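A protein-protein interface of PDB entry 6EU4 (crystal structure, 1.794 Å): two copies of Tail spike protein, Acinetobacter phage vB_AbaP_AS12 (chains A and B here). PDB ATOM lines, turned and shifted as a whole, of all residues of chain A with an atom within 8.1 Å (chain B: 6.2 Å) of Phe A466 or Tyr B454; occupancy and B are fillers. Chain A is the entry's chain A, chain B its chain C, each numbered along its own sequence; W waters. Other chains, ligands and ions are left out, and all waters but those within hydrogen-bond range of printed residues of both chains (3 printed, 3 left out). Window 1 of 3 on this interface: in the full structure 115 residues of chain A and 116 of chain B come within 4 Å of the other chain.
Water W1 lies within hydrogen-bond range of the backbone carbonyl oxygen of Pro B419 (2.7 Å) and the side-chain amino group of Lys A465 (2.9 Å).
Water W2 bridges the backbone carbonyl oxygen (O) of Gly A468 (2.8 Å) and the side-chain hydroxyl (OH) of Tyr B454 (3.0 Å).
Water W3 lies within hydrogen-bond range of the backbone carbonyl oxygen of Pro B419 and the backbone carbonyl oxygen of Lys A465.
Among the printed residues, pairs that only touch across the chains: Lys A465 with Tyr B454 (3.4 Å), Gly A468 with Val B458 (3.4 Å), Phe A466 with Tyr B454 (3.5 Å), Leu A469 with Arg B459 (3.5 Å), Lys A465 with Gly B457 (3.6 Å), Glu A416 with Pro B419 (3.6 Å), Phe A466 with Pro B419 (3.6 Å), Phe A466 with Gly B457 (3.7 Å), Ala A464 with Gly B457 (3.7 Å) and Lys A465 with Pro B419 (3.9 Å).
OG of Ser A450 sits at hydrogen-bond distance from N of Ala A464 (3.2 Å).
The backbone NH of Lys A465 lies within hydrogen-bond range of the side-chain hydroxyl of Ser A450 (3.1 Å).
O of Val B417 sits at hydrogen-bond distance from N of Tyr B454 (3.2 Å).
The side-chain hydroxyl (OG) of Ser B418 lies close to the side-chain carboxylate (OE2) of Glu B420 (3.2 Å).
The guanidinium group (NE) of Arg B459 lies within salt-bridge range of the side-chain carboxylate (OD1) of Asp B452 (2.8 Å).
Hydrophobic or aromatic side chains of chain B within 4 Å of the printed part of chain A: Pro B419, Tyr B454 and Val B458.
Of the 20 printed residues of chain A, 7 touch a printed residue of chain B.
Hydrophobic or aromatic side chains of chain A within 4 Å of the printed part of chain B: Phe A466 and Leu A469.
Among the printed residues, no Asp or Glu carboxylate lies within 4 Å of a Lys or Arg side-chain nitrogen of the other chain.
Positions printed for both chains: 452, 453, 459 and 460.
Of the 14 pairs that touch across the chains among the printed residues, none has its exchanged pair printed and touching as well.
The side-chain carboxylate (OE1) of Glu B420 sits close to the side-chain carboxylate (OE2) of Glu A416, at 2.6 Å.
The backbone NH (N) of Ser A467 lies within hydrogen-bond range of the backbone carbonyl oxygen (O) of Gly B457 (2.7 Å).
The backbone NH (N) of Gly A468 lies within hydrogen-bond range of the backbone carbonyl oxygen (O) of Gly B457 (3.4 Å).
The backbone NH of Arg B459 sits at hydrogen-bond distance from the backbone carbonyl oxygen of Gly A468, 2.9 Å away.
Of chain B, only Pro B419, Tyr B454 and Gly B457 come within 4 Å of Phe A466.
Of chain A, only Lys A465 (3.4 Å) and Phe A466 (3.5 Å) come within 4 Å of Tyr B454.
No residue of chain A comes within 4 Å of Ala B453.
Of the printed residues of chain B, Lys A465 touches Pro B419, Tyr B454 and Gly B457.
Printed residues of chain A within 4 Å of Val B458: Gly A468.
Of the printed residues of chain A, Pro B419 touches Glu A416, Lys A465 and Phe A466.
Val A451 touches none of the printed residues of chain B.
The nearest residue of chain A that does not touch Tyr B454 is Gln A461 (4.1 Å).
The nearest printed residue of chain A that does not touch Glu B420 is Val A414 (4.2 Å).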
ATOM      1  N   SER A 413      -5.224 -10.936 -26.867  1.00  0.00           N
ATOM      2  CA  SER A 413      -6.180  -9.836 -26.901  1.00  0.00           C
ATOM      3  C   SER A 413      -7.100  -9.852 -25.685  1.00  0.00           C
ATOM      4  O   SER A 413      -7.213 -10.846 -24.963  1.00  0.00           O
ATOM      5  CB  SER A 413      -7.022  -9.904 -28.157  1.00  0.00           C
ATOM      6  OG  SER A 413      -6.204  -9.743 -29.312  1.00  0.00           O
ATOM      7  N   VAL A 414      -7.773  -8.728 -25.476  1.00  0.00           N
ATOM      8  CA  VAL A 414      -8.793  -8.594 -24.441  1.00  0.00           C
ATOM      9  C   VAL A 414     -10.004  -7.913 -25.060  1.00  0.00           C
ATOM     10  O   VAL A 414      -9.866  -6.986 -25.868  1.00  0.00           O
ATOM     11  CB  VAL A 414      -8.272  -7.836 -23.206  1.00  0.00           C
ATOM     12  CG1 VAL A 414      -7.835  -6.436 -23.557  1.00  0.00           C
ATOM     13  CG2 VAL A 414      -9.328  -7.826 -22.109  1.00  0.00           C
ATOM     14  N   PHE A 415     -11.187  -8.411 -24.703  1.00  0.00           N
ATOM     15  CA  PHE A 415     -12.470  -7.929 -25.196  1.00  0.00           C
ATOM     16  C   PHE A 415     -13.363  -7.681 -23.990  1.00  0.00           C
ATOM     17  O   PHE A 415     -13.523  -8.569 -23.147  1.00  0.00           O
ATOM     18  CB  PHE A 415     -13.109  -8.966 -26.132  1.00  0.00           C
ATOM     19  CG  PHE A 415     -14.447  -8.568 -26.699  1.00  0.00           C
ATOM     20  CD1 PHE A 415     -14.580  -7.442 -27.506  1.00  0.00           C
ATOM     21  CD2 PHE A 415     -15.567  -9.353 -26.467  1.00  0.00           C
ATOM     22  CE1 PHE A 415     -15.810  -7.105 -28.067  1.00  0.00           C
ATOM     23  CE2 PHE A 415     -16.794  -9.014 -27.016  1.00  0.00           C
ATOM     24  CZ  PHE A 415     -16.919  -7.888 -27.809  1.00  0.00           C
ATOM     25  N   GLU A 416     -13.946  -6.488 -23.912  1.00  0.00           N
ATOM     26  CA  GLU A 416     -14.732  -6.067 -22.757  1.00  0.00           C
ATOM     27  C   GLU A 416     -16.095  -5.586 -23.238  1.00  0.00           C
ATOM     28  O   GLU A 416     -16.177  -4.803 -24.185  1.00  0.00           O
ATOM     29  CB  GLU A 416     -14.005  -4.958 -21.970  1.00  0.00           C
ATOM     30  CG  GLU A 416     -12.644  -5.406 -21.409  1.00  0.00           C
ATOM     31  CD  GLU A 416     -11.707  -4.252 -20.989  1.00  0.00           C
ATOM     32  OE1 GLU A 416     -11.751  -3.155 -21.576  1.00  0.00           O
ATOM     33  OE2 GLU A 416     -10.899  -4.457 -20.072  1.00  0.00           O
ATOM     34  N   ALA A 449      -6.125 -15.497 -24.313  1.00  0.00           N
ATOM     35  CA  ALA A 449      -6.895 -14.278 -24.496  1.00  0.00           C
ATOM     36  C   ALA A 449      -7.611 -14.004 -23.187  1.00  0.00           C
ATOM     37  O   ALA A 449      -7.668 -14.854 -22.293  1.00  0.00           O
ATOM     38  CB  ALA A 449      -7.902 -14.414 -25.643  1.00  0.00           C
ATOM     39  N   SER A 450      -8.153 -12.796 -23.082  1.00  0.00           N
ATOM     40  CA  SER A 450      -8.887 -12.366 -21.906  1.00  0.00           C
ATOM     41  C   SER A 450     -10.219 -11.755 -22.313  1.00  0.00           C
ATOM     42  O   SER A 450     -10.328 -11.098 -23.351  1.00  0.00           O
ATOM     43  CB  SER A 450      -8.089 -11.341 -21.097  1.00  0.00           C
ATOM     44  OG  SER A 450      -6.886 -11.939 -20.568  1.00  0.00           O
ATOM     45  N   VAL A 451     -11.219 -11.955 -21.454  1.00  0.00           N
ATOM     46  CA  VAL A 451     -12.545 -11.383 -21.654  1.00  0.00           C
ATOM     47  C   VAL A 451     -13.078 -10.861 -20.329  1.00  0.00           C
ATOM     48  O   VAL A 451     -12.796 -11.403 -19.256  1.00  0.00           O
ATOM     49  CB  VAL A 451     -13.546 -12.393 -22.254  1.00  0.00           C
ATOM     50  CG1 VAL A 451     -13.113 -12.828 -23.659  1.00  0.00           C
ATOM     51  CG2 VAL A 451     -13.698 -13.608 -21.354  1.00  0.00           C
ATOM     52  N   ASP A 452     -13.875  -9.792 -20.424  1.00  0.00           N
ATOM     53  CA  ASP A 452     -14.629  -9.246 -19.288  1.00  0.00           C
ATOM     54  C   ASP A 452     -15.924  -8.768 -19.919  1.00  0.00           C
ATOM     55  O   ASP A 452     -16.004  -7.644 -20.410  1.00  0.00           O
ATOM     56  CB  ASP A 452     -13.886  -8.136 -18.563  1.00  0.00           C
ATOM     57  CG  ASP A 452     -14.652  -7.593 -17.374  1.00  0.00           C
ATOM     58  OD1 ASP A 452     -15.826  -7.965 -17.197  1.00  0.00           O
ATOM     59  OD2 ASP A 452     -14.074  -6.771 -16.626  1.00  0.00           O
ATOM     60  N   ALA A 453     -16.919  -9.656 -19.962  1.00  0.00           N
ATOM     61  CA  ALA A 453     -18.072  -9.433 -20.817  1.00  0.00           C
ATOM     62  C   ALA A 453     -19.348  -9.888 -20.134  1.00  0.00           C
ATOM     63  O   ALA A 453     -19.449 -11.032 -19.668  1.00  0.00           O
ATOM     64  CB  ALA A 453     -17.936 -10.167 -22.153  1.00  0.00           C
ATOM     65  N   ARG A 459     -21.666 -11.437 -15.659  1.00  0.00           N
ATOM     66  CA  ARG A 459     -20.353 -10.935 -16.026  1.00  0.00           C
ATOM     67  C   ARG A 459     -19.374 -12.100 -16.021  1.00  0.00           C
ATOM     68  O   ARG A 459     -19.206 -12.770 -14.998  1.00  0.00           O
ATOM     69  CB  ARG A 459     -19.897  -9.851 -15.054  1.00  0.00           C
ATOM     70  CG  ARG A 459     -18.609  -9.172 -15.464  1.00  0.00           C
ATOM     71  CD  ARG A 459     -18.221  -8.106 -14.449  1.00  0.00           C
ATOM     72  NE  ARG A 459     -17.107  -7.287 -14.888  1.00  0.00           N
ATOM     73  CZ  ARG A 459     -16.730  -6.164 -14.283  1.00  0.00           C
ATOM     74  NH1 ARG A 459     -17.386  -5.733 -13.198  1.00  0.00           N
ATOM     75  NH2 ARG A 459     -15.697  -5.469 -14.747  1.00  0.00           N
ATOM     76  N   TYR A 460     -18.738 -12.340 -17.162  1.00  0.00           N
ATOM     77  CA  TYR A 460     -17.728 -13.378 -17.311  1.00  0.00           C
ATOM     78  C   TYR A 460     -16.366 -12.722 -17.438  1.00  0.00           C
ATOM     79  O   TYR A 460     -16.148 -11.903 -18.337  1.00  0.00           O
ATOM     80  CB  TYR A 460     -18.026 -14.243 -18.534  1.00  0.00           C
ATOM     81  CG  TYR A 460     -19.308 -15.015 -18.385  1.00  0.00           C
ATOM     82  CD1 TYR A 460     -20.537 -14.463 -18.774  1.00  0.00           C
ATOM     83  CD2 TYR A 460     -19.302 -16.287 -17.820  1.00  0.00           C
ATOM     84  CE1 TYR A 460     -21.710 -15.170 -18.621  1.00  0.00           C
ATOM     85  CE2 TYR A 460     -20.473 -17.000 -17.665  1.00  0.00           C
ATOM     86  CZ  TYR A 460     -21.671 -16.432 -18.058  1.00  0.00           C
ATOM     87  OH  TYR A 460     -22.813 -17.156 -17.887  1.00  0.00           O
ATOM     88  N   GLN A 461     -15.453 -13.088 -16.544  1.00  0.00           N
ATOM     89  CA  GLN A 461     -14.071 -12.640 -16.589  1.00  0.00           C
ATOM     90  C   GLN A 461     -13.154 -13.859 -16.671  1.00  0.00           C
ATOM     91  O   GLN A 461     -13.272 -14.792 -15.861  1.00  0.00           O
ATOM     92  CB  GLN A 461     -13.724 -11.802 -15.350  1.00  0.00           C
ATOM     93  CG  GLN A 461     -14.539 -10.529 -15.199  1.00  0.00           C
ATOM     94  CD  GLN A 461     -14.202  -9.766 -13.933  1.00  0.00           C
ATOM     95  OE1 GLN A 461     -14.205 -10.326 -12.843  1.00  0.00           O
ATOM     96  NE2 GLN A 461     -13.899  -8.489 -14.073  1.00  0.00           N
ATOM     97  N   ASP A 462     -12.236 -13.846 -17.634  1.00  0.00           N
ATOM     98  CA  ASP A 462     -11.299 -14.953 -17.786  1.00  0.00           C
ATOM     99  C   ASP A 462     -10.032 -14.445 -18.461  1.00  0.00           C
ATOM    100  O   ASP A 462     -10.050 -13.457 -19.192  1.00  0.00           O
ATOM    101  CB  ASP A 462     -11.946 -16.071 -18.606  1.00  0.00           C
ATOM    102  CG  ASP A 462     -11.303 -17.436 -18.391  1.00  0.00           C
ATOM    103  OD1 ASP A 462     -10.351 -17.558 -17.597  1.00  0.00           O
ATOM    104  OD2 ASP A 462     -11.778 -18.401 -19.029  1.00  0.00           O
ATOM    105  N   GLY A 463      -8.927 -15.140 -18.228  1.00  0.00           N
ATOM    106  CA  GLY A 463      -7.695 -14.846 -18.930  1.00  0.00           C
ATOM    107  C   GLY A 463      -6.672 -14.183 -18.017  1.00  0.00           C
ATOM    108  O   GLY A 463      -6.947 -13.823 -16.872  1.00  0.00           O
ATOM    109  N   ALA A 464      -5.467 -14.020 -18.568  1.00  0.00           N
ATOM    110  CA  ALA A 464      -4.346 -13.546 -17.755  1.00  0.00           C
ATOM    111  C   ALA A 464      -4.542 -12.121 -17.236  1.00  0.00           C
ATOM    112  O   ALA A 464      -3.927 -11.754 -16.225  1.00  0.00           O
ATOM    113  CB  ALA A 464      -3.049 -13.618 -18.552  1.00  0.00           C
ATOM    114  N   LYS A 465      -5.346 -11.306 -17.902  1.00  0.00           N
ATOM    115  CA  LYS A 465      -5.584  -9.953 -17.413  1.00  0.00           C
ATOM    116  C   LYS A 465      -6.549  -9.928 -16.236  1.00  0.00           C
ATOM    117  O   LYS A 465      -6.705  -8.881 -15.597  1.00  0.00           O
ATOM    118  CB  LYS A 465      -6.104  -9.084 -18.548  1.00  0.00           C
ATOM    119  CG  LYS A 465      -5.045  -8.881 -19.646  1.00  0.00           C
ATOM    120  CD  LYS A 465      -5.402  -7.805 -20.602  1.00  0.00           C
ATOM    121  CE  LYS A 465      -4.313  -7.682 -21.679  1.00  0.00           C
ATOM    122  NZ  LYS A 465      -2.983  -7.313 -21.102  1.00  0.00           N
ATOM    123  N   PHE A 466      -7.180 -11.063 -15.921  1.00  0.00           N
ATOM    124  CA  PHE A 466      -8.176 -11.155 -14.860  1.00  0.00           C
ATOM    125  C   PHE A 466      -7.821 -12.352 -13.990  1.00  0.00           C
ATOM    126  O   PHE A 466      -8.536 -13.362 -13.929  1.00  0.00           O
ATOM    127  CB  PHE A 466      -9.573 -11.267 -15.444  1.00  0.00           C
ATOM    128  CG  PHE A 466      -9.935 -10.122 -16.325  1.00  0.00           C
ATOM    129  CD1 PHE A 466     -10.306  -8.907 -15.773  1.00  0.00           C
ATOM    130  CD2 PHE A 466      -9.880 -10.229 -17.694  1.00  0.00           C
ATOM    131  CE1 PHE A 466     -10.629  -7.852 -16.564  1.00  0.00           C
ATOM    132  CE2 PHE A 466     -10.194  -9.160 -18.489  1.00  0.00           C
ATOM    133  CZ  PHE A 466     -10.559  -7.968 -17.923  1.00  0.00           C
ATOM    134  N   SER A 467      -6.688 -12.246 -13.305  1.00  0.00           N
ATOM    135  CA  SER A 467      -6.175 -13.339 -12.489  1.00  0.00           C
ATOM    136  C   SER A 467      -6.753 -13.343 -11.084  1.00  0.00           C
ATOM    137  O   SER A 467      -6.925 -14.412 -10.489  1.00  0.00           O
ATOM    138  CB  SER A 467      -4.651 -13.251 -12.390  1.00  0.00           C
ATOM    139  OG  SER A 467      -4.145 -14.215 -11.481  1.00  0.00           O
ATOM    140  N   GLY A 468      -7.039 -12.171 -10.536  1.00  0.00           N
ATOM    141  CA  GLY A 468      -7.514 -12.129  -9.163  1.00  0.00           C
ATOM    142  C   GLY A 468      -8.125 -10.785  -8.836  1.00  0.00           C
ATOM    143  O   GLY A 468      -8.011  -9.816  -9.591  1.00  0.00           O
ATOM    144  N   LEU A 469      -8.793 -10.768  -7.682  1.00  0.00           N
ATOM    145  CA  LEU A 469      -9.447  -9.590  -7.118  1.00  0.00           C
ATOM    146  C   LEU A 469      -9.139  -9.578  -5.631  1.00  0.00           C
ATOM    147  O   LEU A 469      -9.481 -10.532  -4.925  1.00  0.00           O
ATOM    148  CB  LEU A 469     -10.960  -9.635  -7.340  1.00  0.00           C
ATOM    149  CG  LEU A 469     -11.777  -8.551  -6.643  1.00  0.00           C
ATOM    150  CD1 LEU A 469     -11.271  -7.153  -6.951  1.00  0.00           C
ATOM    151  CD2 LEU A 469     -13.237  -8.689  -7.080  1.00  0.00           C
ATOM    152  N   VAL B 417      -6.789   2.298 -12.214  1.00  0.00           N
ATOM    153  CA  VAL B 417      -6.094   1.796 -13.400  1.00  0.00           C
ATOM    154  C   VAL B 417      -6.892   0.626 -13.947  1.00  0.00           C
ATOM    155  O   VAL B 417      -7.017  -0.405 -13.273  1.00  0.00           O
ATOM    156  CB  VAL B 417      -4.652   1.349 -13.090  1.00  0.00           C
ATOM    157  CG1 VAL B 417      -3.957   0.845 -14.395  1.00  0.00           C
ATOM    158  CG2 VAL B 417      -3.846   2.474 -12.463  1.00  0.00           C
ATOM    159  N   SER B 418      -7.385   0.761 -15.182  1.00  0.00           N
ATOM    160  CA  SER B 418      -8.178  -0.289 -15.826  1.00  0.00           C
ATOM    161  C   SER B 418      -7.330  -1.540 -16.124  1.00  0.00           C
ATOM    162  O   SER B 418      -6.100  -1.473 -16.220  1.00  0.00           O
ATOM    163  CB  SER B 418      -8.792   0.248 -17.124  1.00  0.00           C
ATOM    164  OG  SER B 418      -7.828   0.292 -18.139  1.00  0.00           O
ATOM    165  N   PRO B 419      -7.979  -2.699 -16.313  1.00  0.00           N
ATOM    166  CA  PRO B 419      -7.211  -3.928 -16.613  1.00  0.00           C
ATOM    167  C   PRO B 419      -6.583  -3.935 -17.987  1.00  0.00           C
ATOM    168  O   PRO B 419      -5.671  -4.744 -18.236  1.00  0.00           O
ATOM    169  CB  PRO B 419      -8.260  -5.041 -16.487  1.00  0.00           C
ATOM    170  CG  PRO B 419      -9.564  -4.374 -16.737  1.00  0.00           C
ATOM    171  CD  PRO B 419      -9.414  -2.982 -16.134  1.00  0.00           C
ATOM    172  N   GLU B 420      -7.050  -3.085 -18.886  1.00  0.00           N
ATOM    173  CA  GLU B 420      -6.530  -3.044 -20.239  1.00  0.00           C
ATOM    174  C   GLU B 420      -5.508  -1.929 -20.457  1.00  0.00           C
ATOM    175  O   GLU B 420      -4.965  -1.823 -21.559  1.00  0.00           O
ATOM    176  CB  GLU B 420      -7.691  -2.933 -21.241  1.00  0.00           C
ATOM    177  CG  GLU B 420      -8.384  -1.595 -21.339  1.00  0.00           C
ATOM    178  CD  GLU B 420      -9.462  -1.339 -20.284  1.00  0.00           C
ATOM    179  OE1 GLU B 420      -9.703  -2.202 -19.409  1.00  0.00           O
ATOM    180  OE2 GLU B 420     -10.103  -0.260 -20.364  1.00  0.00           O
ATOM    181  N   PHE B 423       1.674  -0.954 -20.131  1.00  0.00           N
ATOM    182  CA  PHE B 423       2.908  -0.258 -19.790  1.00  0.00           C
ATOM    183  C   PHE B 423       4.071  -0.907 -20.524  1.00  0.00           C
ATOM    184  O   PHE B 423       4.062  -2.113 -20.778  1.00  0.00           O
ATOM    185  CB  PHE B 423       3.154  -0.294 -18.282  1.00  0.00           C
ATOM    186  CG  PHE B 423       2.031   0.290 -17.493  1.00  0.00           C
ATOM    187  CD1 PHE B 423       1.938   1.654 -17.322  1.00  0.00           C
ATOM    188  CD2 PHE B 423       1.037  -0.521 -16.966  1.00  0.00           C
ATOM    189  CE1 PHE B 423       0.888   2.216 -16.608  1.00  0.00           C
ATOM    190  CE2 PHE B 423      -0.038   0.036 -16.256  1.00  0.00           C
ATOM    191  CZ  PHE B 423      -0.107   1.400 -16.074  1.00  0.00           C
ATOM    192  N   LEU B 427       4.754  -3.317 -14.113  1.00  0.00           N
ATOM    193  CA  LEU B 427       4.591  -2.780 -12.767  1.00  0.00           C
ATOM    194  C   LEU B 427       5.112  -3.785 -11.748  1.00  0.00           C
ATOM    195  O   LEU B 427       5.192  -4.985 -12.006  1.00  0.00           O
ATOM    196  CB  LEU B 427       3.119  -2.478 -12.479  1.00  0.00           C
ATOM    197  CG  LEU B 427       2.378  -1.553 -13.441  1.00  0.00           C
ATOM    198  CD1 LEU B 427       0.983  -1.240 -12.910  1.00  0.00           C
ATOM    199  CD2 LEU B 427       3.155  -0.263 -13.752  1.00  0.00           C
ATOM    200  N   VAL B 443       2.557   1.267  -7.207  1.00  0.00           N
ATOM    201  CA  VAL B 443       1.459   2.137  -6.812  1.00  0.00           C
ATOM    202  C   VAL B 443       1.500   2.246  -5.301  1.00  0.00           C
ATOM    203  O   VAL B 443       1.279   1.252  -4.594  1.00  0.00           O
ATOM    204  CB  VAL B 443       0.108   1.600  -7.281  1.00  0.00           C
ATOM    205  CG1 VAL B 443      -1.025   2.483  -6.745  1.00  0.00           C
ATOM    206  CG2 VAL B 443       0.057   1.562  -8.792  1.00  0.00           C
ATOM    207  N   ASP B 452      -8.111   1.626  -6.959  1.00  0.00           N
ATOM    208  CA  ASP B 452      -8.766   0.518  -7.660  1.00  0.00           C
ATOM    209  C   ASP B 452      -7.893   0.317  -8.891  1.00  0.00           C
ATOM    210  O   ASP B 452      -8.097   0.974  -9.916  1.00  0.00           O
ATOM    211  CB  ASP B 452     -10.211   0.848  -8.005  1.00  0.00           C
ATOM    212  CG  ASP B 452     -10.944  -0.296  -8.698  1.00  0.00           C
ATOM    213  OD1 ASP B 452     -10.302  -1.281  -9.084  1.00  0.00           O
ATOM    214  OD2 ASP B 452     -12.171  -0.184  -8.887  1.00  0.00           O
ATOM    215  N   ALA B 453      -6.882  -0.539  -8.762  1.00  0.00           N
ATOM    216  CA  ALA B 453      -5.859  -0.673  -9.784  1.00  0.00           C
ATOM    217  C   ALA B 453      -5.530  -2.126 -10.058  1.00  0.00           C
ATOM    218  O   ALA B 453      -5.288  -2.908  -9.135  1.00  0.00           O
ATOM    219  CB  ALA B 453      -4.572   0.046  -9.383  1.00  0.00           C
ATOM    220  N   TYR B 454      -5.481  -2.473 -11.338  1.00  0.00           N
ATOM    221  CA  TYR B 454      -4.904  -3.739 -11.750  1.00  0.00           C
ATOM    222  C   TYR B 454      -3.395  -3.647 -11.712  1.00  0.00           C
ATOM    223  O   TYR B 454      -2.804  -2.693 -12.240  1.00  0.00           O
ATOM    224  CB  TYR B 454      -5.366  -4.116 -13.159  1.00  0.00           C
ATOM    225  CG  TYR B 454      -6.667  -4.830 -13.145  1.00  0.00           C
ATOM    226  CD1 TYR B 454      -7.852  -4.131 -13.080  1.00  0.00           C
ATOM    227  CD2 TYR B 454      -6.709  -6.217 -13.155  1.00  0.00           C
ATOM    228  CE1 TYR B 454      -9.058  -4.790 -13.047  1.00  0.00           C
ATOM    229  CE2 TYR B 454      -7.898  -6.881 -13.127  1.00  0.00           C
ATOM    230  CZ  TYR B 454      -9.062  -6.170 -13.069  1.00  0.00           C
ATOM    231  OH  TYR B 454     -10.263  -6.811 -13.031  1.00  0.00           O
ATOM    232  N   VAL B 455      -2.777  -4.644 -11.091  1.00  0.00           N
ATOM    233  CA  VAL B 455      -1.335  -4.816 -11.084  1.00  0.00           C
ATOM    234  C   VAL B 455      -1.036  -6.285 -11.335  1.00  0.00           C
ATOM    235  O   VAL B 455      -1.398  -7.147 -10.526  1.00  0.00           O
ATOM    236  CB  VAL B 455      -0.704  -4.351  -9.762  1.00  0.00           C
ATOM    237  CG1 VAL B 455       0.782  -4.597  -9.778  1.00  0.00           C
ATOM    238  CG2 VAL B 455      -1.029  -2.865  -9.546  1.00  0.00           C
ATOM    239  N   LYS B 456      -0.349  -6.569 -12.444  1.00  0.00           N
ATOM    240  CA  LYS B 456       0.009  -7.939 -12.829  1.00  0.00           C
ATOM    241  C   LYS B 456      -1.219  -8.851 -12.869  1.00  0.00           C
ATOM    242  O   LYS B 456      -1.177 -10.008 -12.443  1.00  0.00           O
ATOM    243  CB  LYS B 456       1.083  -8.494 -11.906  1.00  0.00           C
ATOM    244  CG  LYS B 456       2.381  -7.717 -12.013  1.00  0.00           C
ATOM    245  CD  LYS B 456       3.546  -8.445 -11.380  1.00  0.00           C
ATOM    246  CE  LYS B 456       3.732  -8.030  -9.946  1.00  0.00           C
ATOM    247  NZ  LYS B 456       5.061  -8.450  -9.373  1.00  0.00           N
ATOM    248  N   GLY B 457      -2.314  -8.317 -13.400  1.00  0.00           N
ATOM    249  CA  GLY B 457      -3.525  -9.080 -13.629  1.00  0.00           C
ATOM    250  C   GLY B 457      -4.406  -9.242 -12.410  1.00  0.00           C
ATOM    251  O   GLY B 457      -5.402  -9.978 -12.469  1.00  0.00           O
ATOM    252  N   VAL B 458      -4.067  -8.585 -11.306  1.00  0.00           N
ATOM    253  CA  VAL B 458      -4.837  -8.657 -10.065  1.00  0.00           C
ATOM    254  C   VAL B 458      -5.376  -7.271  -9.768  1.00  0.00           C
ATOM    255  O   VAL B 458      -4.619  -6.291  -9.776  1.00  0.00           O
ATOM    256  CB  VAL B 458      -3.984  -9.175  -8.893  1.00  0.00           C
ATOM    257  CG1 VAL B 458      -4.809  -9.216  -7.616  1.00  0.00           C
ATOM    258  CG2 VAL B 458      -3.427 -10.543  -9.201  1.00  0.00           C
ATOM    259  N   ARG B 459      -6.676  -7.192  -9.519  1.00  0.00           N
ATOM    260  CA  ARG B 459      -7.347  -5.943  -9.199  1.00  0.00           C
ATOM    261  C   ARG B 459      -7.236  -5.724  -7.701  1.00  0.00           C
ATOM    262  O   ARG B 459      -7.606  -6.608  -6.923  1.00  0.00           O
ATOM    263  CB  ARG B 459      -8.817  -5.999  -9.605  1.00  0.00           C
ATOM    264  CG  ARG B 459      -9.566  -4.679  -9.461  1.00  0.00           C
ATOM    265  CD  ARG B 459     -10.962  -4.795 -10.020  1.00  0.00           C
ATOM    266  NE  ARG B 459     -11.641  -3.511 -10.065  1.00  0.00           N
ATOM    267  CZ  ARG B 459     -12.816  -3.306 -10.660  1.00  0.00           C
ATOM    268  NH1 ARG B 459     -13.473  -4.317 -11.247  1.00  0.00           N
ATOM    269  NH2 ARG B 459     -13.362  -2.094 -10.637  1.00  0.00           N
ATOM    270  N   TYR B 460      -6.712  -4.566  -7.305  1.00  0.00           N
ATOM    271  CA  TYR B 460      -6.573  -4.198  -5.900  1.00  0.00           C
ATOM    272  C   TYR B 460      -7.482  -3.019  -5.608  1.00  0.00           C
ATOM    273  O   TYR B 460      -7.374  -1.966  -6.250  1.00  0.00           O
ATOM    274  CB  TYR B 460      -5.130  -3.843  -5.547  1.00  0.00           C
ATOM    275  CG  TYR B 460      -4.182  -4.998  -5.664  1.00  0.00           C
ATOM    276  CD1 TYR B 460      -3.566  -5.291  -6.875  1.00  0.00           C
ATOM    277  CD2 TYR B 460      -3.914  -5.814  -4.576  1.00  0.00           C
ATOM    278  CE1 TYR B 460      -2.703  -6.350  -6.989  1.00  0.00           C
ATOM    279  CE2 TYR B 460      -3.053  -6.879  -4.689  1.00  0.00           C
ATOM    280  CZ  TYR B 460      -2.449  -7.141  -5.909  1.00  0.00           C
ATOM    281  OH  TYR B 460      -1.596  -8.209  -6.027  1.00  0.00           O
HETATM  282  O   HOH W   1      -3.345  -4.765 -19.673  1.00  0.00           O
HETATM  283  O   HOH W   2      -9.549  -9.503 -11.918  1.00  0.00           O
HETATM  284  O   HOH W   3      -4.853  -6.669 -16.213  1.00  0.00           O
